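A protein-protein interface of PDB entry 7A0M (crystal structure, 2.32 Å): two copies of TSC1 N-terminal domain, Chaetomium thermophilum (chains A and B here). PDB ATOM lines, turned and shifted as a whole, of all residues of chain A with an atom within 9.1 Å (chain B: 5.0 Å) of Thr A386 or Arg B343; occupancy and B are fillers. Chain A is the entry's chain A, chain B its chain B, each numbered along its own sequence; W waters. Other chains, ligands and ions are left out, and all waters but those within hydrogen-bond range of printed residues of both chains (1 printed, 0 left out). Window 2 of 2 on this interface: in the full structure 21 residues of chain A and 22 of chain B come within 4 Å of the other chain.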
ATOM      1  N   TYR A 334     -19.479   2.056 -13.923  1.00  0.00           N
ATOM      2  CA  TYR A 334     -20.443   3.157 -13.980  1.00  0.00           C
ATOM      3  C   TYR A 334     -19.729   4.470 -13.686  1.00  0.00           C
ATOM      4  O   TYR A 334     -19.937   5.093 -12.639  1.00  0.00           O
ATOM      5  CB  TYR A 334     -21.599   2.915 -13.007  1.00  0.00           C
ATOM      6  CG  TYR A 334     -22.468   1.738 -13.392  1.00  0.00           C
ATOM      7  CD1 TYR A 334     -23.573   1.909 -14.216  1.00  0.00           C
ATOM      8  CD2 TYR A 334     -22.181   0.456 -12.941  1.00  0.00           C
ATOM      9  CE1 TYR A 334     -24.370   0.838 -14.578  1.00  0.00           C
ATOM     10  CE2 TYR A 334     -22.971  -0.622 -13.298  1.00  0.00           C
ATOM     11  CZ  TYR A 334     -24.064  -0.424 -14.117  1.00  0.00           C
ATOM     12  OH  TYR A 334     -24.856  -1.490 -14.477  1.00  0.00           O
ATOM     13  N   PRO A 335     -18.874   4.928 -14.610  1.00  0.00           N
ATOM     14  CA  PRO A 335     -18.111   6.164 -14.351  1.00  0.00           C
ATOM     15  C   PRO A 335     -18.970   7.410 -14.231  1.00  0.00           C
ATOM     16  O   PRO A 335     -18.740   8.228 -13.330  1.00  0.00           O
ATOM     17  CB  PRO A 335     -17.175   6.247 -15.564  1.00  0.00           C
ATOM     18  CG  PRO A 335     -17.890   5.493 -16.636  1.00  0.00           C
ATOM     19  CD  PRO A 335     -18.572   4.359 -15.933  1.00  0.00           C
ATOM     20  N   ILE A 336     -19.947   7.586 -15.123  1.00  0.00           N
ATOM     21  CA  ILE A 336     -20.740   8.813 -15.124  1.00  0.00           C
ATOM     22  C   ILE A 336     -21.552   8.928 -13.841  1.00  0.00           C
ATOM     23  O   ILE A 336     -21.659  10.009 -13.250  1.00  0.00           O
ATOM     24  CB  ILE A 336     -21.636   8.869 -16.376  1.00  0.00           C
ATOM     25  CG1 ILE A 336     -20.781   8.760 -17.641  1.00  0.00           C
ATOM     26  CG2 ILE A 336     -22.446  10.156 -16.397  1.00  0.00           C
ATOM     27  CD1 ILE A 336     -21.584   8.706 -18.920  1.00  0.00           C
ATOM     28  N   ASN A 337     -22.134   7.817 -13.385  1.00  0.00           N
ATOM     29  CA  ASN A 337     -22.852   7.832 -12.115  1.00  0.00           C
ATOM     30  C   ASN A 337     -21.903   7.995 -10.935  1.00  0.00           C
ATOM     31  O   ASN A 337     -22.265   8.626  -9.935  1.00  0.00           O
ATOM     32  CB  ASN A 337     -23.677   6.555 -11.959  1.00  0.00           C
ATOM     33  CG  ASN A 337     -24.936   6.569 -12.802  1.00  0.00           C
ATOM     34  OD1 ASN A 337     -26.008   6.937 -12.328  1.00  0.00           O
ATOM     35  ND2 ASN A 337     -24.809   6.168 -14.061  1.00  0.00           N
ATOM     36  N   ASP A 340     -20.693  11.582 -10.707  1.00  0.00           N
ATOM     37  CA  ASP A 340     -21.835  12.384 -10.288  1.00  0.00           C
ATOM     38  C   ASP A 340     -22.111  12.216  -8.801  1.00  0.00           C
ATOM     39  O   ASP A 340     -22.542  13.166  -8.139  1.00  0.00           O
ATOM     40  CB  ASP A 340     -23.072  12.014 -11.105  1.00  0.00           C
ATOM     41  CG  ASP A 340     -24.225  12.972 -10.882  1.00  0.00           C
ATOM     42  OD1 ASP A 340     -24.187  14.088 -11.442  1.00  0.00           O
ATOM     43  OD2 ASP A 340     -25.171  12.608 -10.151  1.00  0.00           O
ATOM     44  N   PRO A 380     -14.383   5.944 -21.730  1.00  0.00           N
ATOM     45  CA  PRO A 380     -15.121   6.017 -23.004  1.00  0.00           C
ATOM     46  C   PRO A 380     -16.621   6.222 -22.842  1.00  0.00           C
ATOM     47  O   PRO A 380     -17.267   6.676 -23.795  1.00  0.00           O
ATOM     48  CB  PRO A 380     -14.805   4.671 -23.674  1.00  0.00           C
ATOM     49  CG  PRO A 380     -14.338   3.781 -22.565  1.00  0.00           C
ATOM     50  CD  PRO A 380     -13.636   4.682 -21.598  1.00  0.00           C
ATOM     51  N   ASN A 381     -17.197   5.893 -21.681  1.00  0.00           N
ATOM     52  CA  ASN A 381     -18.624   6.130 -21.470  1.00  0.00           C
ATOM     53  C   ASN A 381     -18.971   7.602 -21.628  1.00  0.00           C
ATOM     54  O   ASN A 381     -20.099   7.938 -22.009  1.00  0.00           O
ATOM     55  CB  ASN A 381     -19.051   5.641 -20.087  1.00  0.00           C
ATOM     56  CG  ASN A 381     -19.279   4.147 -20.040  1.00  0.00           C
ATOM     57  OD1 ASN A 381     -18.768   3.399 -20.875  1.00  0.00           O
ATOM     58  ND2 ASN A 381     -20.057   3.703 -19.061  1.00  0.00           N
ATOM     59  N   PHE A 382     -18.020   8.489 -21.337  1.00  0.00           N
ATOM     60  CA  PHE A 382     -18.243   9.923 -21.459  1.00  0.00           C
ATOM     61  C   PHE A 382     -18.421  10.364 -22.908  1.00  0.00           C
ATOM     62  O   PHE A 382     -18.863  11.494 -23.140  1.00  0.00           O
ATOM     63  CB  PHE A 382     -17.093  10.687 -20.799  1.00  0.00           C
ATOM     64  CG  PHE A 382     -17.092  10.597 -19.295  1.00  0.00           C
ATOM     65  CD1 PHE A 382     -17.998  11.329 -18.542  1.00  0.00           C
ATOM     66  CD2 PHE A 382     -16.193   9.774 -18.635  1.00  0.00           C
ATOM     67  CE1 PHE A 382     -18.002  11.244 -17.160  1.00  0.00           C
ATOM     68  CE2 PHE A 382     -16.195   9.685 -17.255  1.00  0.00           C
ATOM     69  CZ  PHE A 382     -17.099  10.421 -16.518  1.00  0.00           C
ATOM     70  N   TYR A 383     -18.090   9.510 -23.878  1.00  0.00           N
ATOM     71  CA  TYR A 383     -18.354   9.779 -25.284  1.00  0.00           C
ATOM     72  C   TYR A 383     -19.638   9.138 -25.773  1.00  0.00           C
ATOM     73  O   TYR A 383     -19.992   9.315 -26.940  1.00  0.00           O
ATOM     74  CB  TYR A 383     -17.241   9.191 -26.159  1.00  0.00           C
ATOM     75  CG  TYR A 383     -15.875   9.820 -26.110  1.00  0.00           C
ATOM     76  CD1 TYR A 383     -15.659  11.054 -25.522  1.00  0.00           C
ATOM     77  CD2 TYR A 383     -14.786   9.157 -26.657  1.00  0.00           C
ATOM     78  CE1 TYR A 383     -14.391  11.611 -25.487  1.00  0.00           C
ATOM     79  CE2 TYR A 383     -13.525   9.702 -26.625  1.00  0.00           C
ATOM     80  CZ  TYR A 383     -13.332  10.927 -26.041  1.00  0.00           C
ATOM     81  OH  TYR A 383     -12.067  11.459 -26.019  1.00  0.00           O
ATOM     82  N   GLU A 384     -20.366   8.435 -24.917  1.00  0.00           N
ATOM     83  CA  GLU A 384     -21.396   7.554 -25.448  1.00  0.00           C
ATOM     84  C   GLU A 384     -22.717   7.650 -24.701  1.00  0.00           C
ATOM     85  O   GLU A 384     -23.785   7.479 -25.296  1.00  0.00           O
ATOM     86  CB  GLU A 384     -20.888   6.110 -25.425  1.00  0.00           C
ATOM     87  CG  GLU A 384     -20.790   5.447 -26.783  1.00  0.00           C
ATOM     88  CD  GLU A 384     -19.819   4.282 -26.779  1.00  0.00           C
ATOM     89  OE1 GLU A 384     -18.794   4.364 -26.071  1.00  0.00           O
ATOM     90  OE2 GLU A 384     -20.086   3.278 -27.469  1.00  0.00           O
ATOM     91  N   TYR A 385     -22.659   7.923 -23.401  1.00  0.00           N
ATOM     92  CA  TYR A 385     -23.827   7.777 -22.556  1.00  0.00           C
ATOM     93  C   TYR A 385     -24.076   9.041 -21.755  1.00  0.00           C
ATOM     94  O   TYR A 385     -23.186   9.871 -21.552  1.00  0.00           O
ATOM     95  CB  TYR A 385     -23.655   6.596 -21.588  1.00  0.00           C
ATOM     96  CG  TYR A 385     -23.305   5.304 -22.284  1.00  0.00           C
ATOM     97  CD1 TYR A 385     -24.272   4.563 -22.947  1.00  0.00           C
ATOM     98  CD2 TYR A 385     -22.003   4.827 -22.286  1.00  0.00           C
ATOM     99  CE1 TYR A 385     -23.948   3.381 -23.593  1.00  0.00           C
ATOM    100  CE2 TYR A 385     -21.672   3.648 -22.926  1.00  0.00           C
ATOM    101  CZ  TYR A 385     -22.649   2.930 -23.578  1.00  0.00           C
ATOM    102  OH  TYR A 385     -22.322   1.757 -24.218  1.00  0.00           O
ATOM    103  N   THR A 386     -25.317   9.167 -21.310  1.00  0.00           N
ATOM    104  CA  THR A 386     -25.696  10.091 -20.262  1.00  0.00           C
ATOM    105  C   THR A 386     -25.683   9.329 -18.943  1.00  0.00           C
ATOM    106  O   THR A 386     -25.403   8.129 -18.894  1.00  0.00           O
ATOM    107  CB  THR A 386     -27.068  10.702 -20.547  1.00  0.00           C
ATOM    108  OG1 THR A 386     -28.068   9.676 -20.498  1.00  0.00           O
ATOM    109  CG2 THR A 386     -27.084  11.351 -21.920  1.00  0.00           C
ATOM    110  N   ILE A 387     -25.987  10.037 -17.854  1.00  0.00           N
ATOM    111  CA  ILE A 387     -26.056   9.374 -16.560  1.00  0.00           C
ATOM    112  C   ILE A 387     -27.197   8.363 -16.517  1.00  0.00           C
ATOM    113  O   ILE A 387     -27.146   7.409 -15.732  1.00  0.00           O
ATOM    114  CB  ILE A 387     -26.175  10.427 -15.442  1.00  0.00           C
ATOM    115  CG1 ILE A 387     -26.051   9.774 -14.064  1.00  0.00           C
ATOM    116  CG2 ILE A 387     -27.479  11.206 -15.571  1.00  0.00           C
ATOM    117  CD1 ILE A 387     -26.025  10.764 -12.925  1.00  0.00           C
ATOM    118  N   GLU A 388     -28.213   8.528 -17.366  1.00  0.00           N
ATOM    119  CA  GLU A 388     -29.340   7.601 -17.376  1.00  0.00           C
ATOM    120  C   GLU A 388     -29.051   6.375 -18.237  1.00  0.00           C
ATOM    121  O   GLU A 388     -29.182   5.237 -17.772  1.00  0.00           O
ATOM    122  CB  GLU A 388     -30.606   8.306 -17.869  1.00  0.00           C
ATOM    123  CG  GLU A 388     -31.035   9.503 -17.033  1.00  0.00           C
ATOM    124  CD  GLU A 388     -30.341  10.786 -17.446  1.00  0.00           C
ATOM    125  OE1 GLU A 388     -29.583  10.759 -18.438  1.00  0.00           O
ATOM    126  OE2 GLU A 388     -30.553  11.820 -16.779  1.00  0.00           O
ATOM    127  N   THR A 389     -28.659   6.587 -19.497  1.00  0.00           N
ATOM    128  CA  THR A 389     -28.452   5.466 -20.410  1.00  0.00           C
ATOM    129  C   THR A 389     -27.260   4.604 -20.016  1.00  0.00           C
ATOM    130  O   THR A 389     -27.197   3.440 -20.424  1.00  0.00           O
ATOM    131  CB  THR A 389     -28.273   5.967 -21.844  1.00  0.00           C
ATOM    132  OG1 THR A 389     -27.232   6.950 -21.885  1.00  0.00           O
ATOM    133  CG2 THR A 389     -29.568   6.579 -22.360  1.00  0.00           C
ATOM    134  N   GLU A 390     -26.316   5.142 -19.242  1.00  0.00           N
ATOM    135  CA  GLU A 390     -25.234   4.313 -18.722  1.00  0.00           C
ATOM    136  C   GLU A 390     -25.774   3.176 -17.861  1.00  0.00           C
ATOM    137  O   GLU A 390     -25.267   2.049 -17.916  1.00  0.00           O
ATOM    138  CB  GLU A 390     -24.258   5.167 -17.917  1.00  0.00           C
ATOM    139  CG  GLU A 390     -23.154   4.367 -17.252  1.00  0.00           C
ATOM    140  CD  GLU A 390     -22.190   5.238 -16.482  1.00  0.00           C
ATOM    141  OE1 GLU A 390     -21.188   5.678 -17.078  1.00  0.00           O
ATOM    142  OE2 GLU A 390     -22.441   5.489 -15.284  1.00  0.00           O
ATOM    143  N   LYS A 391     -26.810   3.449 -17.069  1.00  0.00           N
ATOM    144  CA  LYS A 391     -27.422   2.402 -16.262  1.00  0.00           C
ATOM    145  C   LYS A 391     -28.419   1.579 -17.062  1.00  0.00           C
ATOM    146  O   LYS A 391     -28.618   0.394 -16.772  1.00  0.00           O
ATOM    147  CB  LYS A 391     -28.122   3.017 -15.050  1.00  0.00           C
ATOM    148  CG  LYS A 391     -27.197   3.729 -14.079  1.00  0.00           C
ATOM    149  CD  LYS A 391     -27.987   4.366 -12.946  1.00  0.00           C
ATOM    150  CE  LYS A 391     -28.925   5.447 -13.465  1.00  0.00           C
ATOM    151  NZ  LYS A 391     -29.620   6.158 -12.356  1.00  0.00           N
ATOM    152  N   THR A 392     -29.044   2.185 -18.069  1.00  0.00           N
ATOM    153  CA  THR A 392     -30.136   1.547 -18.788  1.00  0.00           C
ATOM    154  C   THR A 392     -29.663   0.759 -20.007  1.00  0.00           C
ATOM    155  O   THR A 392     -30.184  -0.329 -20.278  1.00  0.00           O
ATOM    156  CB  THR A 392     -31.162   2.607 -19.197  1.00  0.00           C
ATOM    157  OG1 THR A 392     -31.991   2.929 -18.073  1.00  0.00           O
ATOM    158  CG2 THR A 392     -32.026   2.096 -20.305  1.00  0.00           C
ATOM    159  N   ASN A 393     -28.665   1.260 -20.732  1.00  0.00           N
ATOM    160  CA  ASN A 393     -28.184   0.570 -21.921  1.00  0.00           C
ATOM    161  C   ASN A 393     -27.239  -0.540 -21.479  1.00  0.00           C
ATOM    162  O   ASN A 393     -26.222  -0.274 -20.830  1.00  0.00           O
ATOM    163  CB  ASN A 393     -27.484   1.545 -22.869  1.00  0.00           C
ATOM    164  CG  ASN A 393     -27.273   0.968 -24.259  1.00  0.00           C
ATOM    165  OD1 ASN A 393     -26.999  -0.221 -24.420  1.00  0.00           O
ATOM    166  ND2 ASN A 393     -27.398   1.817 -25.273  1.00  0.00           N
ATOM    167  N   ARG A 396     -23.157  -2.880 -23.439  1.00  0.00           N
ATOM    168  CA  ARG A 396     -21.806  -3.085 -22.923  1.00  0.00           C
ATOM    169  C   ARG A 396     -21.626  -4.483 -22.344  1.00  0.00           C
ATOM    170  O   ARG A 396     -20.570  -5.101 -22.513  1.00  0.00           O
ATOM    171  CB  ARG A 396     -21.458  -2.051 -21.852  1.00  0.00           C
ATOM    172  CG  ARG A 396     -21.089  -0.671 -22.358  1.00  0.00           C
ATOM    173  CD  ARG A 396     -20.718   0.218 -21.179  1.00  0.00           C
ATOM    174  NE  ARG A 396     -21.827   0.439 -20.257  1.00  0.00           N
ATOM    175  CZ  ARG A 396     -21.669   0.766 -18.979  1.00  0.00           C
ATOM    176  NH1 ARG A 396     -20.448   0.892 -18.476  1.00  0.00           N
ATOM    177  NH2 ARG A 396     -22.724   0.954 -18.197  1.00  0.00           N
ATOM    178  N   VAL B 339     -16.619  16.673 -24.265  1.00  0.00           N
ATOM    179  CA  VAL B 339     -17.003  15.271 -24.401  1.00  0.00           C
ATOM    180  C   VAL B 339     -18.482  15.149 -24.742  1.00  0.00           C
ATOM    181  O   VAL B 339     -18.902  14.161 -25.356  1.00  0.00           O
ATOM    182  CB  VAL B 339     -16.645  14.481 -23.128  1.00  0.00           C
ATOM    183  CG1 VAL B 339     -15.172  14.658 -22.785  1.00  0.00           C
ATOM    184  CG2 VAL B 339     -17.529  14.901 -21.960  1.00  0.00           C
ATOM    185  N   ASP B 340     -19.294  16.140 -24.361  1.00  0.00           N
ATOM    186  CA  ASP B 340     -20.694  16.136 -24.772  1.00  0.00           C
ATOM    187  C   ASP B 340     -20.839  16.401 -26.264  1.00  0.00           C
ATOM    188  O   ASP B 340     -21.758  15.871 -26.899  1.00  0.00           O
ATOM    189  CB  ASP B 340     -21.487  17.167 -23.970  1.00  0.00           C
ATOM    190  CG  ASP B 340     -22.983  17.042 -24.184  1.00  0.00           C
ATOM    191  OD1 ASP B 340     -23.593  16.118 -23.603  1.00  0.00           O
ATOM    192  OD2 ASP B 340     -23.549  17.866 -24.932  1.00  0.00           O
ATOM    193  N   TYR B 341     -19.955  17.223 -26.839  1.00  0.00           N
ATOM    194  CA  TYR B 341     -19.954  17.401 -28.287  1.00  0.00           C
ATOM    195  C   TYR B 341     -19.606  16.095 -28.988  1.00  0.00           C
ATOM    196  O   TYR B 341     -20.246  15.718 -29.976  1.00  0.00           O
ATOM    197  CB  TYR B 341     -18.970  18.505 -28.680  1.00  0.00           C
ATOM    198  CG  TYR B 341     -18.802  18.685 -30.174  1.00  0.00           C
ATOM    199  CD1 TYR B 341     -19.695  19.459 -30.903  1.00  0.00           C
ATOM    200  CD2 TYR B 341     -17.748  18.087 -30.853  1.00  0.00           C
ATOM    201  CE1 TYR B 341     -19.548  19.630 -32.267  1.00  0.00           C
ATOM    202  CE2 TYR B 341     -17.593  18.252 -32.218  1.00  0.00           C
ATOM    203  CZ  TYR B 341     -18.494  19.025 -32.920  1.00  0.00           C
ATOM    204  OH  TYR B 341     -18.343  19.192 -34.277  1.00  0.00           O
ATOM    205  N   ILE B 342     -18.585  15.394 -28.490  1.00  0.00           N
ATOM    206  CA  ILE B 342     -18.219  14.100 -29.056  1.00  0.00           C
ATOM    207  C   ILE B 342     -19.326  13.079 -28.823  1.00  0.00           C
ATOM    208  O   ILE B 342     -19.571  12.213 -29.673  1.00  0.00           O
ATOM    209  CB  ILE B 342     -16.877  13.628 -28.465  1.00  0.00           C
ATOM    210  CG1 ILE B 342     -15.759  14.604 -28.832  1.00  0.00           C
ATOM    211  CG2 ILE B 342     -16.531  12.223 -28.944  1.00  0.00           C
ATOM    212  CD1 ILE B 342     -14.427  14.271 -28.195  1.00  0.00           C
ATOM    213  N   ARG B 343     -20.026  13.171 -27.690  1.00  0.00           N
ATOM    214  CA  ARG B 343     -21.089  12.214 -27.402  1.00  0.00           C
ATOM    215  C   ARG B 343     -22.284  12.418 -28.321  1.00  0.00           C
ATOM    216  O   ARG B 343     -22.811  11.458 -28.894  1.00  0.00           O
ATOM    217  CB  ARG B 343     -21.543  12.336 -25.947  1.00  0.00           C
ATOM    218  CG  ARG B 343     -22.677  11.379 -25.603  1.00  0.00           C
ATOM    219  CD  ARG B 343     -23.276  11.658 -24.237  1.00  0.00           C
ATOM    220  NE  ARG B 343     -23.920  12.968 -24.187  1.00  0.00           N
ATOM    221  CZ  ARG B 343     -25.182  13.195 -24.544  1.00  0.00           C
ATOM    222  NH1 ARG B 343     -25.938  12.197 -24.984  1.00  0.00           N
ATOM    223  NH2 ARG B 343     -25.689  14.417 -24.466  1.00  0.00           N
ATOM    224  N   LYS B 344     -22.725  13.662 -28.474  1.00  0.00           N
ATOM    225  CA  LYS B 344     -23.939  13.973 -29.226  1.00  0.00           C
ATOM    226  C   LYS B 344     -23.684  15.207 -30.074  1.00  0.00           C
ATOM    227  O   LYS B 344     -24.081  16.322 -29.717  1.00  0.00           O
ATOM    228  CB  LYS B 344     -25.130  14.173 -28.284  1.00  0.00           C
ATOM    229  CG  LYS B 344     -26.487  14.169 -28.969  1.00  0.00           C
ATOM    230  CD  LYS B 344     -27.580  14.638 -28.020  1.00  0.00           C
ATOM    231  CE  LYS B 344     -28.949  14.569 -28.676  1.00  0.00           C
ATOM    232  NZ  LYS B 344     -29.981  15.302 -27.891  1.00  0.00           N
ATOM    233  N   PRO B 345     -23.015  15.043 -31.219  1.00  0.00           N
ATOM    234  CA  PRO B 345     -22.860  16.177 -32.140  1.00  0.00           C
ATOM    235  C   PRO B 345     -24.143  16.514 -32.866  1.00  0.00           C
ATOM    236  O   PRO B 345     -24.176  17.503 -33.613  1.00  0.00           O
ATOM    237  CB  PRO B 345     -21.779  15.692 -33.111  1.00  0.00           C
ATOM    238  CG  PRO B 345     -21.970  14.213 -33.145  1.00  0.00           C
ATOM    239  CD  PRO B 345     -22.402  13.812 -31.751  1.00  0.00           C
ATOM    240  N   ASN B 347     -26.581  17.758 -31.337  1.00  0.00           N
ATOM    241  CA  ASN B 347     -26.934  19.027 -30.709  1.00  0.00           C
ATOM    242  C   ASN B 347     -26.259  20.234 -31.351  1.00  0.00           C
ATOM    243  O   ASN B 347     -26.608  21.368 -31.005  1.00  0.00           O
ATOM    244  CB  ASN B 347     -26.579  18.986 -29.220  1.00  0.00           C
ATOM    245  CG  ASN B 347     -27.565  18.172 -28.408  1.00  0.00           C
ATOM    246  OD1 ASN B 347     -28.556  17.671 -28.938  1.00  0.00           O
ATOM    247  ND2 ASN B 347     -27.297  18.034 -27.114  1.00  0.00           N
ATOM    248  N   ARG B 366     -16.070   9.673 -32.578  1.00  0.00           N
ATOM    249  CA  ARG B 366     -15.693   8.976 -31.351  1.00  0.00           C
ATOM    250  C   ARG B 366     -14.504   8.055 -31.582  1.00  0.00           C
ATOM    251  O   ARG B 366     -13.542   8.057 -30.805  1.00  0.00           O
ATOM    252  CB  ARG B 366     -16.883   8.181 -30.817  1.00  0.00           C
ATOM    253  CG  ARG B 366     -17.951   9.016 -30.156  1.00  0.00           C
ATOM    254  CD  ARG B 366     -18.932   8.122 -29.431  1.00  0.00           C
ATOM    255  NE  ARG B 366     -19.949   7.564 -30.315  1.00  0.00           N
ATOM    256  CZ  ARG B 366     -21.171   8.068 -30.450  1.00  0.00           C
ATOM    257  NH1 ARG B 366     -21.526   9.142 -29.757  1.00  0.00           N
ATOM    258  NH2 ARG B 366     -22.037   7.499 -31.275  1.00  0.00           N
HETATM  259  O   HOH W   1     -25.648   9.590 -25.880  1.00  0.00           O
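The backbone carbonyl oxygen of Val B339 sits close to the backbone carbonyl oxygen of Phe A382, at 3.5 Å.
O of Tyr A383 lies close to NH1 of Arg B366 (3.2 Å).
The backbone carbonyl oxygen (O) of Arg B343 is in hydrogen-bond range of the guanidinium group (NH1) of Arg B366 (2.8 Å).
OG1 of Thr A386 lies within hydrogen-bond range of OE1 of Glu A388.
The side-chain carboxylate (OD1) of Asp B340 is in salt-bridge range of the guanidinium group (NH2) of Arg B343 (2.8 Å).
N of Thr A386 sits at hydrogen-bond distance from OG1 of Thr A389 (3.0 Å).
O of Phe A382 touches CB of Arg B343, 3.97 Å away.
Ile B342 touches Tyr A383 (CG2 to CD1, 3.7 Å).
Tyr A383 touches Arg B343 (O to CA, 3.1 Å).
Glu A384 touches Arg B343.
Tyr A385 touches Arg B343.
CG2 of Thr A386 touches NH1 of Arg B343, 3.4 Å away.
Of the printed residues of chain B, Tyr A383 touches Ile B342 (3.7 Å), Arg B343 (3.1 Å) and Arg B366 (3.0 Å).
Thr A386 touches just one residue of chain B: Arg B343 (3.4 Å).
Of the printed residues of chain A, Val B339 touches Phe A382.
Arg B343 touches just these residues of chain A: Phe A382 (3.97 Å), Tyr A383 (3.1 Å), Glu A384 (3.8 Å), Tyr A385 (3.2 Å) and Thr A386 (3.4 Å).
Lys B344 touches none of the printed residues of chain A.
Asn B347 touches none of the printed residues of chain A.
Printed residues of chain A within 4 Å of Arg B366: Tyr A383.
The nearest printed residue of chain B that does not touch Thr A386 is Asp B340 (6.1 Å).
Hydrophobic or aromatic side chains of chain A within 4 Å of the printed part of chain B: Tyr A383.
Printed residues of chain B that touch a printed residue of chain A: Val B339, Ile B342, Arg B343 and Arg B366.
1 position is printed for both chains.
Water W1 lies within hydrogen-bond range of the guanidinium group of Arg B343 (2.8 Å) and the backbone carbonyl oxygen of Glu A384 (2.9 Å).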
